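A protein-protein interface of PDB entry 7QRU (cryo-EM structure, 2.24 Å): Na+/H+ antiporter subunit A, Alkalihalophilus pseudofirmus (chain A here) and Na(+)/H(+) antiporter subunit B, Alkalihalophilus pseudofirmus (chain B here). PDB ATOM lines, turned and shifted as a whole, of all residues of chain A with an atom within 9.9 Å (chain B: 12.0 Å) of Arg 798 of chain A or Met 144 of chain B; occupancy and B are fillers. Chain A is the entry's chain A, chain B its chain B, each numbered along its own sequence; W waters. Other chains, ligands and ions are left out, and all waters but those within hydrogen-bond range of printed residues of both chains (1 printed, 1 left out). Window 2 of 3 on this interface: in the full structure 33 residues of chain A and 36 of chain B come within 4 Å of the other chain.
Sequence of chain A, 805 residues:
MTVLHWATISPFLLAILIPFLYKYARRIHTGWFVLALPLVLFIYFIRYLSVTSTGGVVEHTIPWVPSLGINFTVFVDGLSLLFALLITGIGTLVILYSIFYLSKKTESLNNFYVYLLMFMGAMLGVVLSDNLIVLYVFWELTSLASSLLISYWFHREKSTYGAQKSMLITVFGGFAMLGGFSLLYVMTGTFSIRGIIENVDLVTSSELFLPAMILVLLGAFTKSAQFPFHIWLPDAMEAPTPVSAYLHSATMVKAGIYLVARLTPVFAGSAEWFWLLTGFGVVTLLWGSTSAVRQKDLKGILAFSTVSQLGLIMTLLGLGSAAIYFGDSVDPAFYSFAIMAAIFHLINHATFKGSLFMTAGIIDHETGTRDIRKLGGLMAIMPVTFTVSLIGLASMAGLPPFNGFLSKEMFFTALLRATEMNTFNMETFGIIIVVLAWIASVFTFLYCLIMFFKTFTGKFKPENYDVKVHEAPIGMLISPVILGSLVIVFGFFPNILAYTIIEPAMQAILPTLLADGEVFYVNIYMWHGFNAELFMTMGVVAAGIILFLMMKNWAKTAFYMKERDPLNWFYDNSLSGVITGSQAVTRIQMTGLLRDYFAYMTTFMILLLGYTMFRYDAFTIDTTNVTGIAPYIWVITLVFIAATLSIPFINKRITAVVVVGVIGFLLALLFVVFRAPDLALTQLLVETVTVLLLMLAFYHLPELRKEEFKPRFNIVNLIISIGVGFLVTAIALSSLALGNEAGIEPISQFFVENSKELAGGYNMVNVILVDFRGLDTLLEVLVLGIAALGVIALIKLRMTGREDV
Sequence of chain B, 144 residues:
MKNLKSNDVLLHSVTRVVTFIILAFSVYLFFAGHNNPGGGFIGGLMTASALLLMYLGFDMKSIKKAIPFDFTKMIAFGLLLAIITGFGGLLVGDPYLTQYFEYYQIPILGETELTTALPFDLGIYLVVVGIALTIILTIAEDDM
Of the 9 printed residues of chain B, 4 touch a printed residue of chain A. Of the 15 printed residues of chain A, 4 touch a printed residue of chain B. Among the printed residues, Asp or Glu carboxylates within 4 Å of a Lys or Arg side-chain nitrogen of the other chain: Arg 798 of chain A with Asp 142 of chain B.
The backbone NH (N) of Met 144 of chain B sits close to the side-chain carboxylate (OD1) of Asp 142 of chain B, at 3.4 Å. The backbone carbonyl oxygen (O) of Ile 795 of chain A is in hydrogen-bond range of the guanidinium group (NH2) of Arg 798 of chain A (2.9 Å).
Of chain B, only Asp 142 and Met 144 come within 4 Å of Arg 798 of chain A. Of chain A, only Ile 795 and Arg 798 come within 4 Å of Met 144 of chain B. Ile 795 of chain A touches just these residues of chain B: Thr 138, Ile 139, Asp 142 and Met 144. No residue of chain B comes within 4 Å of Thr 800 of chain A. Of the printed residues of chain A, Ile 139 of chain B touches Ile 795. Of the printed residues of chain A, Thr 138 of chain B touches Ile 792 (3.98 Å) and Ile 795 (3.8 Å). Of the printed residues of chain B, Ile 792 of chain A touches Thr 138 (3.98 Å). Tyr 699 of chain A touches none of the printed residues of chain B. Val 791 of chain A touches none of the printed residues of chain B. The nearest printed residue of chain A that does not touch Met 144 of chain B is Lys 796 of chain A (4.9 Å).
Water W1 lies within hydrogen-bond range of O of Ile 139 of chain B (2.5 Å), NE2 of His 700 of chain A (3.1 Å) and O of Ala 140 of chain B (3.3 Å).
The guanidinium group (NH2) of Arg 798 of chain A lies within salt-bridge range of the side-chain carboxylate (OD1) of Asp 142 of chain B (3.3 Å). The guanidinium group of Arg 798 of chain A is in salt-bridge range of the chain-end carboxylate of Met 144 of chain B (3.0 Å).
Among the printed residues, pairs that only touch across the chains: His 700 of chain A with Asp 142 of chain B, Ile 795 of chain A with Asp 142 of chain B, Ile 795 of chain A with Thr 138 of chain B, Ile 795 of chain A with Met 144 of chain B, Ile 795 of chain A with Ile 139 of chain B and Ile 792 of chain A with Thr 138 of chain B.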
ATOM      1  N   TYR A 699       4.399   0.719 -12.872  1.00  0.00           N
ATOM      2  CA  TYR A 699       3.314   1.543 -13.341  1.00  0.00           C
ATOM      3  C   TYR A 699       3.822   2.956 -13.740  1.00  0.00           C
ATOM      4  O   TYR A 699       3.150   3.686 -14.466  1.00  0.00           O
ATOM      5  CB  TYR A 699       2.214   1.521 -12.290  1.00  0.00           C
ATOM      6  CG  TYR A 699       1.107   2.521 -12.566  1.00  0.00           C
ATOM      7  CD1 TYR A 699       1.041   3.787 -11.973  1.00  0.00           C
ATOM      8  CD2 TYR A 699       0.108   2.180 -13.446  1.00  0.00           C
ATOM      9  CE1 TYR A 699       0.026   4.684 -12.277  1.00  0.00           C
ATOM     10  CE2 TYR A 699      -0.921   3.058 -13.738  1.00  0.00           C
ATOM     11  CZ  TYR A 699      -0.962   4.316 -13.165  1.00  0.00           C
ATOM     12  OH  TYR A 699      -1.962   5.216 -13.434  1.00  0.00           O
ATOM     13  N   HIS A 700       4.964   3.371 -13.192  1.00  0.00           N
ATOM     14  CA  HIS A 700       5.476   4.721 -13.320  1.00  0.00           C
ATOM     15  C   HIS A 700       6.613   4.729 -14.320  1.00  0.00           C
ATOM     16  O   HIS A 700       6.603   5.544 -15.227  1.00  0.00           O
ATOM     17  CB  HIS A 700       5.914   5.180 -11.938  1.00  0.00           C
ATOM     18  CG  HIS A 700       4.753   5.526 -11.072  1.00  0.00           C
ATOM     19  ND1 HIS A 700       3.971   6.675 -11.285  1.00  0.00           N
ATOM     20  CD2 HIS A 700       4.330   4.929  -9.932  1.00  0.00           C
ATOM     21  CE1 HIS A 700       3.072   6.707 -10.303  1.00  0.00           C
ATOM     22  NE2 HIS A 700       3.274   5.657  -9.432  1.00  0.00           N
ATOM     23  N   VAL A 791       9.882   7.772   1.805  1.00  0.00           N
ATOM     24  CA  VAL A 791       9.044   7.488   0.686  1.00  0.00           C
ATOM     25  C   VAL A 791       7.836   8.416   0.749  1.00  0.00           C
ATOM     26  O   VAL A 791       7.528   8.986  -0.319  1.00  0.00           O
ATOM     27  CB  VAL A 791       8.607   6.001   0.604  1.00  0.00           C
ATOM     28  CG1 VAL A 791       7.432   5.755  -0.316  1.00  0.00           C
ATOM     29  CG2 VAL A 791       9.804   5.198   0.202  1.00  0.00           C
ATOM     30  N   ILE A 792       7.203   8.603   1.912  1.00  0.00           N
ATOM     31  CA  ILE A 792       6.083   9.563   1.900  1.00  0.00           C
ATOM     32  C   ILE A 792       6.571  10.932   1.407  1.00  0.00           C
ATOM     33  O   ILE A 792       5.901  11.567   0.613  1.00  0.00           O
ATOM     34  CB  ILE A 792       5.437   9.709   3.293  1.00  0.00           C
ATOM     35  CG1 ILE A 792       4.788   8.411   3.739  1.00  0.00           C
ATOM     36  CG2 ILE A 792       4.437  10.862   3.369  1.00  0.00           C
ATOM     37  CD1 ILE A 792       4.516   8.454   5.233  1.00  0.00           C
ATOM     38  N   ALA A 793       7.682  11.450   1.962  1.00  0.00           N
ATOM     39  CA  ALA A 793       8.121  12.797   1.639  1.00  0.00           C
ATOM     40  C   ALA A 793       8.417  12.874   0.154  1.00  0.00           C
ATOM     41  O   ALA A 793       8.041  13.771  -0.521  1.00  0.00           O
ATOM     42  CB  ALA A 793       9.358  13.109   2.498  1.00  0.00           C
ATOM     43  N   LEU A 794       9.118  11.892  -0.380  1.00  0.00           N
ATOM     44  CA  LEU A 794       9.464  11.891  -1.784  1.00  0.00           C
ATOM     45  C   LEU A 794       8.231  11.835  -2.674  1.00  0.00           C
ATOM     46  O   LEU A 794       8.253  12.429  -3.673  1.00  0.00           O
ATOM     47  CB  LEU A 794      10.371  10.716  -1.934  1.00  0.00           C
ATOM     48  CG  LEU A 794      11.240  10.576  -3.141  1.00  0.00           C
ATOM     49  CD1 LEU A 794      11.887  11.877  -3.540  1.00  0.00           C
ATOM     50  CD2 LEU A 794      12.255   9.522  -2.760  1.00  0.00           C
ATOM     51  N   ILE A 795       7.152  11.180  -2.323  1.00  0.00           N
ATOM     52  CA  ILE A 795       5.981  11.149  -3.167  1.00  0.00           C
ATOM     53  C   ILE A 795       5.113  12.398  -2.934  1.00  0.00           C
ATOM     54  O   ILE A 795       4.744  13.034  -3.838  1.00  0.00           O
ATOM     55  CB  ILE A 795       5.239   9.811  -2.943  1.00  0.00           C
ATOM     56  CG1 ILE A 795       5.939   8.697  -3.690  1.00  0.00           C
ATOM     57  CG2 ILE A 795       3.815   9.899  -3.372  1.00  0.00           C
ATOM     58  CD1 ILE A 795       5.562   7.375  -3.214  1.00  0.00           C
ATOM     59  N   LYS A 796       4.854  12.827  -1.747  1.00  0.00           N
ATOM     60  CA  LYS A 796       3.928  13.917  -1.481  1.00  0.00           C
ATOM     61  C   LYS A 796       4.527  15.331  -1.505  1.00  0.00           C
ATOM     62  O   LYS A 796       3.800  16.240  -1.829  1.00  0.00           O
ATOM     63  CB  LYS A 796       3.290  13.637  -0.126  1.00  0.00           C
ATOM     64  CG  LYS A 796       2.576  12.280  -0.191  1.00  0.00           C
ATOM     65  CD  LYS A 796       1.646  12.078   0.862  1.00  0.00           C
ATOM     66  CE  LYS A 796       1.024  10.711   0.940  1.00  0.00           C
ATOM     67  NZ  LYS A 796       0.426  10.522   2.299  1.00  0.00           N
ATOM     68  N   LEU A 797       5.814  15.597  -1.251  1.00  0.00           N
ATOM     69  CA  LEU A 797       6.245  16.992  -1.229  1.00  0.00           C
ATOM     70  C   LEU A 797       6.865  17.359  -2.547  1.00  0.00           C
ATOM     71  O   LEU A 797       7.883  16.766  -2.868  1.00  0.00           O
ATOM     72  CB  LEU A 797       7.252  17.254  -0.115  1.00  0.00           C
ATOM     73  CG  LEU A 797       7.886  18.646  -0.140  1.00  0.00           C
ATOM     74  CD1 LEU A 797       6.857  19.716   0.051  1.00  0.00           C
ATOM     75  CD2 LEU A 797       8.855  18.746   0.967  1.00  0.00           C
ATOM     76  N   ARG A 798       6.279  18.315  -3.303  1.00  0.00           N
ATOM     77  CA  ARG A 798       6.810  18.733  -4.635  1.00  0.00           C
ATOM     78  C   ARG A 798       6.798  20.250  -4.661  1.00  0.00           C
ATOM     79  O   ARG A 798       5.766  20.888  -4.428  1.00  0.00           O
ATOM     80  CB  ARG A 798       6.013  18.153  -5.816  1.00  0.00           C
ATOM     81  CG  ARG A 798       5.457  16.764  -5.453  1.00  0.00           C
ATOM     82  CD  ARG A 798       5.071  16.002  -6.666  1.00  0.00           C
ATOM     83  NE  ARG A 798       5.011  14.612  -6.322  1.00  0.00           N
ATOM     84  CZ  ARG A 798       4.470  13.674  -7.099  1.00  0.00           C
ATOM     85  NH1 ARG A 798       4.051  14.077  -8.287  1.00  0.00           N
ATOM     86  NH2 ARG A 798       4.322  12.410  -6.649  1.00  0.00           N
ATOM     87  N   MET A 799       8.002  20.762  -4.625  1.00  0.00           N
ATOM     88  CA  MET A 799       8.364  22.136  -4.398  1.00  0.00           C
ATOM     89  C   MET A 799       8.947  22.605  -5.718  1.00  0.00           C
ATOM     90  O   MET A 799       9.332  21.754  -6.546  1.00  0.00           O
ATOM     91  CB  MET A 799       9.408  22.183  -3.290  1.00  0.00           C
ATOM     92  CG  MET A 799       8.763  22.028  -1.964  1.00  0.00           C
ATOM     93  SD  MET A 799       9.963  22.238  -0.603  1.00  0.00           S
ATOM     94  CE  MET A 799       9.908  24.010  -0.452  1.00  0.00           C
ATOM     95  N   THR A 800       8.880  23.918  -5.982  1.00  0.00           N
ATOM     96  CA  THR A 800       9.382  24.465  -7.248  1.00  0.00           C
ATOM     97  C   THR A 800      10.851  24.847  -7.174  1.00  0.00           C
ATOM     98  O   THR A 800      11.519  24.845  -8.205  1.00  0.00           O
ATOM     99  CB  THR A 800       8.521  25.634  -7.703  1.00  0.00           C
ATOM    100  OG1 THR A 800       8.108  26.427  -6.602  1.00  0.00           O
ATOM    101  CG2 THR A 800       7.237  25.166  -8.348  1.00  0.00           C
ATOM    102  N   GLY A 801      11.349  25.100  -5.970  1.00  0.00           N
ATOM    103  CA  GLY A 801      12.687  25.626  -5.803  1.00  0.00           C
ATOM    104  C   GLY A 801      12.710  27.129  -5.511  1.00  0.00           C
ATOM    105  O   GLY A 801      13.749  27.635  -5.078  1.00  0.00           O
ATOM    106  N   ARG A 802      11.575  27.829  -5.669  1.00  0.00           N
ATOM    107  CA  ARG A 802      11.558  29.249  -5.342  1.00  0.00           C
ATOM    108  C   ARG A 802      10.996  29.543  -3.934  1.00  0.00           C
ATOM    109  O   ARG A 802      10.854  30.703  -3.543  1.00  0.00           O
ATOM    110  CB  ARG A 802      10.841  30.046  -6.442  1.00  0.00           C
ATOM    111  CG  ARG A 802       9.454  29.585  -6.848  1.00  0.00           C
ATOM    112  CD  ARG A 802       8.974  30.291  -8.120  1.00  0.00           C
ATOM    113  NE  ARG A 802       8.420  29.404  -9.155  1.00  0.00           N
ATOM    114  CZ  ARG A 802       9.141  28.591  -9.936  1.00  0.00           C
ATOM    115  NH1 ARG A 802      10.462  28.560  -9.834  1.00  0.00           N
ATOM    116  NH2 ARG A 802       8.537  27.801 -10.814  1.00  0.00           N
ATOM    117  N   GLU A 803      10.759  28.521  -3.125  1.00  0.00           N
ATOM    118  CA  GLU A 803      10.079  28.681  -1.862  1.00  0.00           C
ATOM    119  C   GLU A 803      11.040  29.028  -0.718  1.00  0.00           C
ATOM    120  O   GLU A 803      10.602  29.568   0.310  1.00  0.00           O
ATOM    121  CB  GLU A 803       9.398  27.379  -1.435  1.00  0.00           C
ATOM    122  CG  GLU A 803       8.377  26.843  -2.392  1.00  0.00           C
ATOM    123  CD  GLU A 803       8.889  25.771  -3.342  1.00  0.00           C
ATOM    124  OE1 GLU A 803       8.011  25.112  -4.023  1.00  0.00           O
ATOM    125  OE2 GLU A 803      10.162  25.616  -3.470  1.00  0.00           O
ATOM    126  N   ILE B 135       5.032   2.063   2.942  1.00  0.00           N
ATOM    127  CA  ILE B 135       5.715   2.104   1.658  1.00  0.00           C
ATOM    128  C   ILE B 135       4.819   1.624   0.528  1.00  0.00           C
ATOM    129  O   ILE B 135       4.685   2.337  -0.456  1.00  0.00           O
ATOM    130  CB  ILE B 135       7.005   1.335   1.638  1.00  0.00           C
ATOM    131  CG1 ILE B 135       7.978   2.096   2.528  1.00  0.00           C
ATOM    132  CG2 ILE B 135       7.433   1.219   0.235  1.00  0.00           C
ATOM    133  CD1 ILE B 135       9.161   1.341   2.993  1.00  0.00           C
ATOM    134  N   LEU B 137       1.492   1.173   0.288  1.00  0.00           N
ATOM    135  CA  LEU B 137       0.271   1.902   0.056  1.00  0.00           C
ATOM    136  C   LEU B 137       0.519   3.315  -0.450  1.00  0.00           C
ATOM    137  O   LEU B 137      -0.355   3.879  -1.046  1.00  0.00           O
ATOM    138  CB  LEU B 137      -0.517   1.923   1.359  1.00  0.00           C
ATOM    139  CG  LEU B 137      -1.162   0.589   1.780  1.00  0.00           C
ATOM    140  CD1 LEU B 137      -2.144   0.853   2.895  1.00  0.00           C
ATOM    141  CD2 LEU B 137      -1.862  -0.092   0.660  1.00  0.00           C
ATOM    142  N   THR B 138       1.668   3.907  -0.184  1.00  0.00           N
ATOM    143  CA  THR B 138       1.877   5.291  -0.551  1.00  0.00           C
ATOM    144  C   THR B 138       2.176   5.328  -2.020  1.00  0.00           C
ATOM    145  O   THR B 138       1.634   6.172  -2.692  1.00  0.00           O
ATOM    146  CB  THR B 138       3.037   5.919   0.227  1.00  0.00           C
ATOM    147  OG1 THR B 138       2.677   5.805   1.598  1.00  0.00           O
ATOM    148  CG2 THR B 138       3.268   7.354  -0.183  1.00  0.00           C
ATOM    149  N   ILE B 139       2.940   4.333  -2.485  1.00  0.00           N
ATOM    150  CA  ILE B 139       3.199   4.170  -3.895  1.00  0.00           C
ATOM    151  C   ILE B 139       1.915   3.812  -4.635  1.00  0.00           C
ATOM    152  O   ILE B 139       1.596   4.459  -5.597  1.00  0.00           O
ATOM    153  CB  ILE B 139       4.272   3.123  -4.179  1.00  0.00           C
ATOM    154  CG1 ILE B 139       5.554   3.447  -3.459  1.00  0.00           C
ATOM    155  CG2 ILE B 139       4.512   3.041  -5.653  1.00  0.00           C
ATOM    156  CD1 ILE B 139       6.542   2.295  -3.525  1.00  0.00           C
ATOM    157  N   ALA B 140       1.178   2.817  -4.219  1.00  0.00           N
ATOM    158  CA  ALA B 140      -0.019   2.384  -4.939  1.00  0.00           C
ATOM    159  C   ALA B 140      -1.037   3.521  -5.058  1.00  0.00           C
ATOM    160  O   ALA B 140      -1.682   3.657  -6.068  1.00  0.00           O
ATOM    161  CB  ALA B 140      -0.645   1.218  -4.178  1.00  0.00           C
ATOM    162  N   GLU B 141      -1.164   4.355  -4.061  1.00  0.00           N
ATOM    163  CA  GLU B 141      -2.065   5.477  -4.153  1.00  0.00           C
ATOM    164  C   GLU B 141      -1.464   6.751  -4.745  1.00  0.00           C
ATOM    165  O   GLU B 141      -2.093   7.801  -4.609  1.00  0.00           O
ATOM    166  CB  GLU B 141      -2.494   5.914  -2.754  1.00  0.00           C
ATOM    167  CG  GLU B 141      -3.225   4.822  -2.008  1.00  0.00           C
ATOM    168  CD  GLU B 141      -3.257   4.993  -0.495  1.00  0.00           C
ATOM    169  OE1 GLU B 141      -2.215   5.434   0.091  1.00  0.00           O
ATOM    170  OE2 GLU B 141      -4.302   4.615   0.107  1.00  0.00           O
ATOM    171  N   ASP B 142      -0.212   6.740  -5.219  1.00  0.00           N
ATOM    172  CA  ASP B 142       0.416   7.892  -5.861  1.00  0.00           C
ATOM    173  C   ASP B 142      -0.284   8.160  -7.198  1.00  0.00           C
ATOM    174  O   ASP B 142       0.042   7.554  -8.226  1.00  0.00           O
ATOM    175  CB  ASP B 142       1.929   7.728  -6.071  1.00  0.00           C
ATOM    176  CG  ASP B 142       2.555   8.936  -6.774  1.00  0.00           C
ATOM    177  OD1 ASP B 142       1.959  10.099  -6.641  1.00  0.00           O
ATOM    178  OD2 ASP B 142       3.620   8.756  -7.481  1.00  0.00           O
ATOM    179  N   ASP B 143      -1.204   9.141  -7.173  1.00  0.00           N
ATOM    180  CA  ASP B 143      -1.913   9.617  -8.355  1.00  0.00           C
ATOM    181  C   ASP B 143      -0.960  10.349  -9.289  1.00  0.00           C
ATOM    182  O   ASP B 143      -0.762   9.885 -10.420  1.00  0.00           O
ATOM    183  CB  ASP B 143      -3.087  10.508  -7.955  1.00  0.00           C
ATOM    184  CG  ASP B 143      -3.983   9.810  -6.945  1.00  0.00           C
ATOM    185  OD1 ASP B 143      -4.259   8.612  -7.165  1.00  0.00           O
ATOM    186  OD2 ASP B 143      -4.364  10.445  -5.930  1.00  0.00           O
ATOM    187  N   MET B 144      -0.307  11.397  -8.743  1.00  0.00           N
ATOM    188  CA  MET B 144       0.524  12.352  -9.481  1.00  0.00           C
ATOM    189  C   MET B 144       1.805  11.682 -10.039  1.00  0.00           C
ATOM    190  O   MET B 144       1.794  11.337 -11.255  1.00  0.00           O
ATOM    191  CB  MET B 144       0.939  13.532  -8.588  1.00  0.00           C
ATOM    192  CG  MET B 144      -0.127  14.069  -7.631  1.00  0.00           C
ATOM    193  SD  MET B 144       0.565  14.493  -5.962  1.00  0.00           S
ATOM    194  CE  MET B 144       1.171  12.901  -5.384  1.00  0.00           C
ATOM    195  OXT MET B 144       2.802  11.539  -9.269  1.00  0.00           O
HETATM  196  O   HOH W   1       0.928   4.139  -7.980  1.00  0.00           O
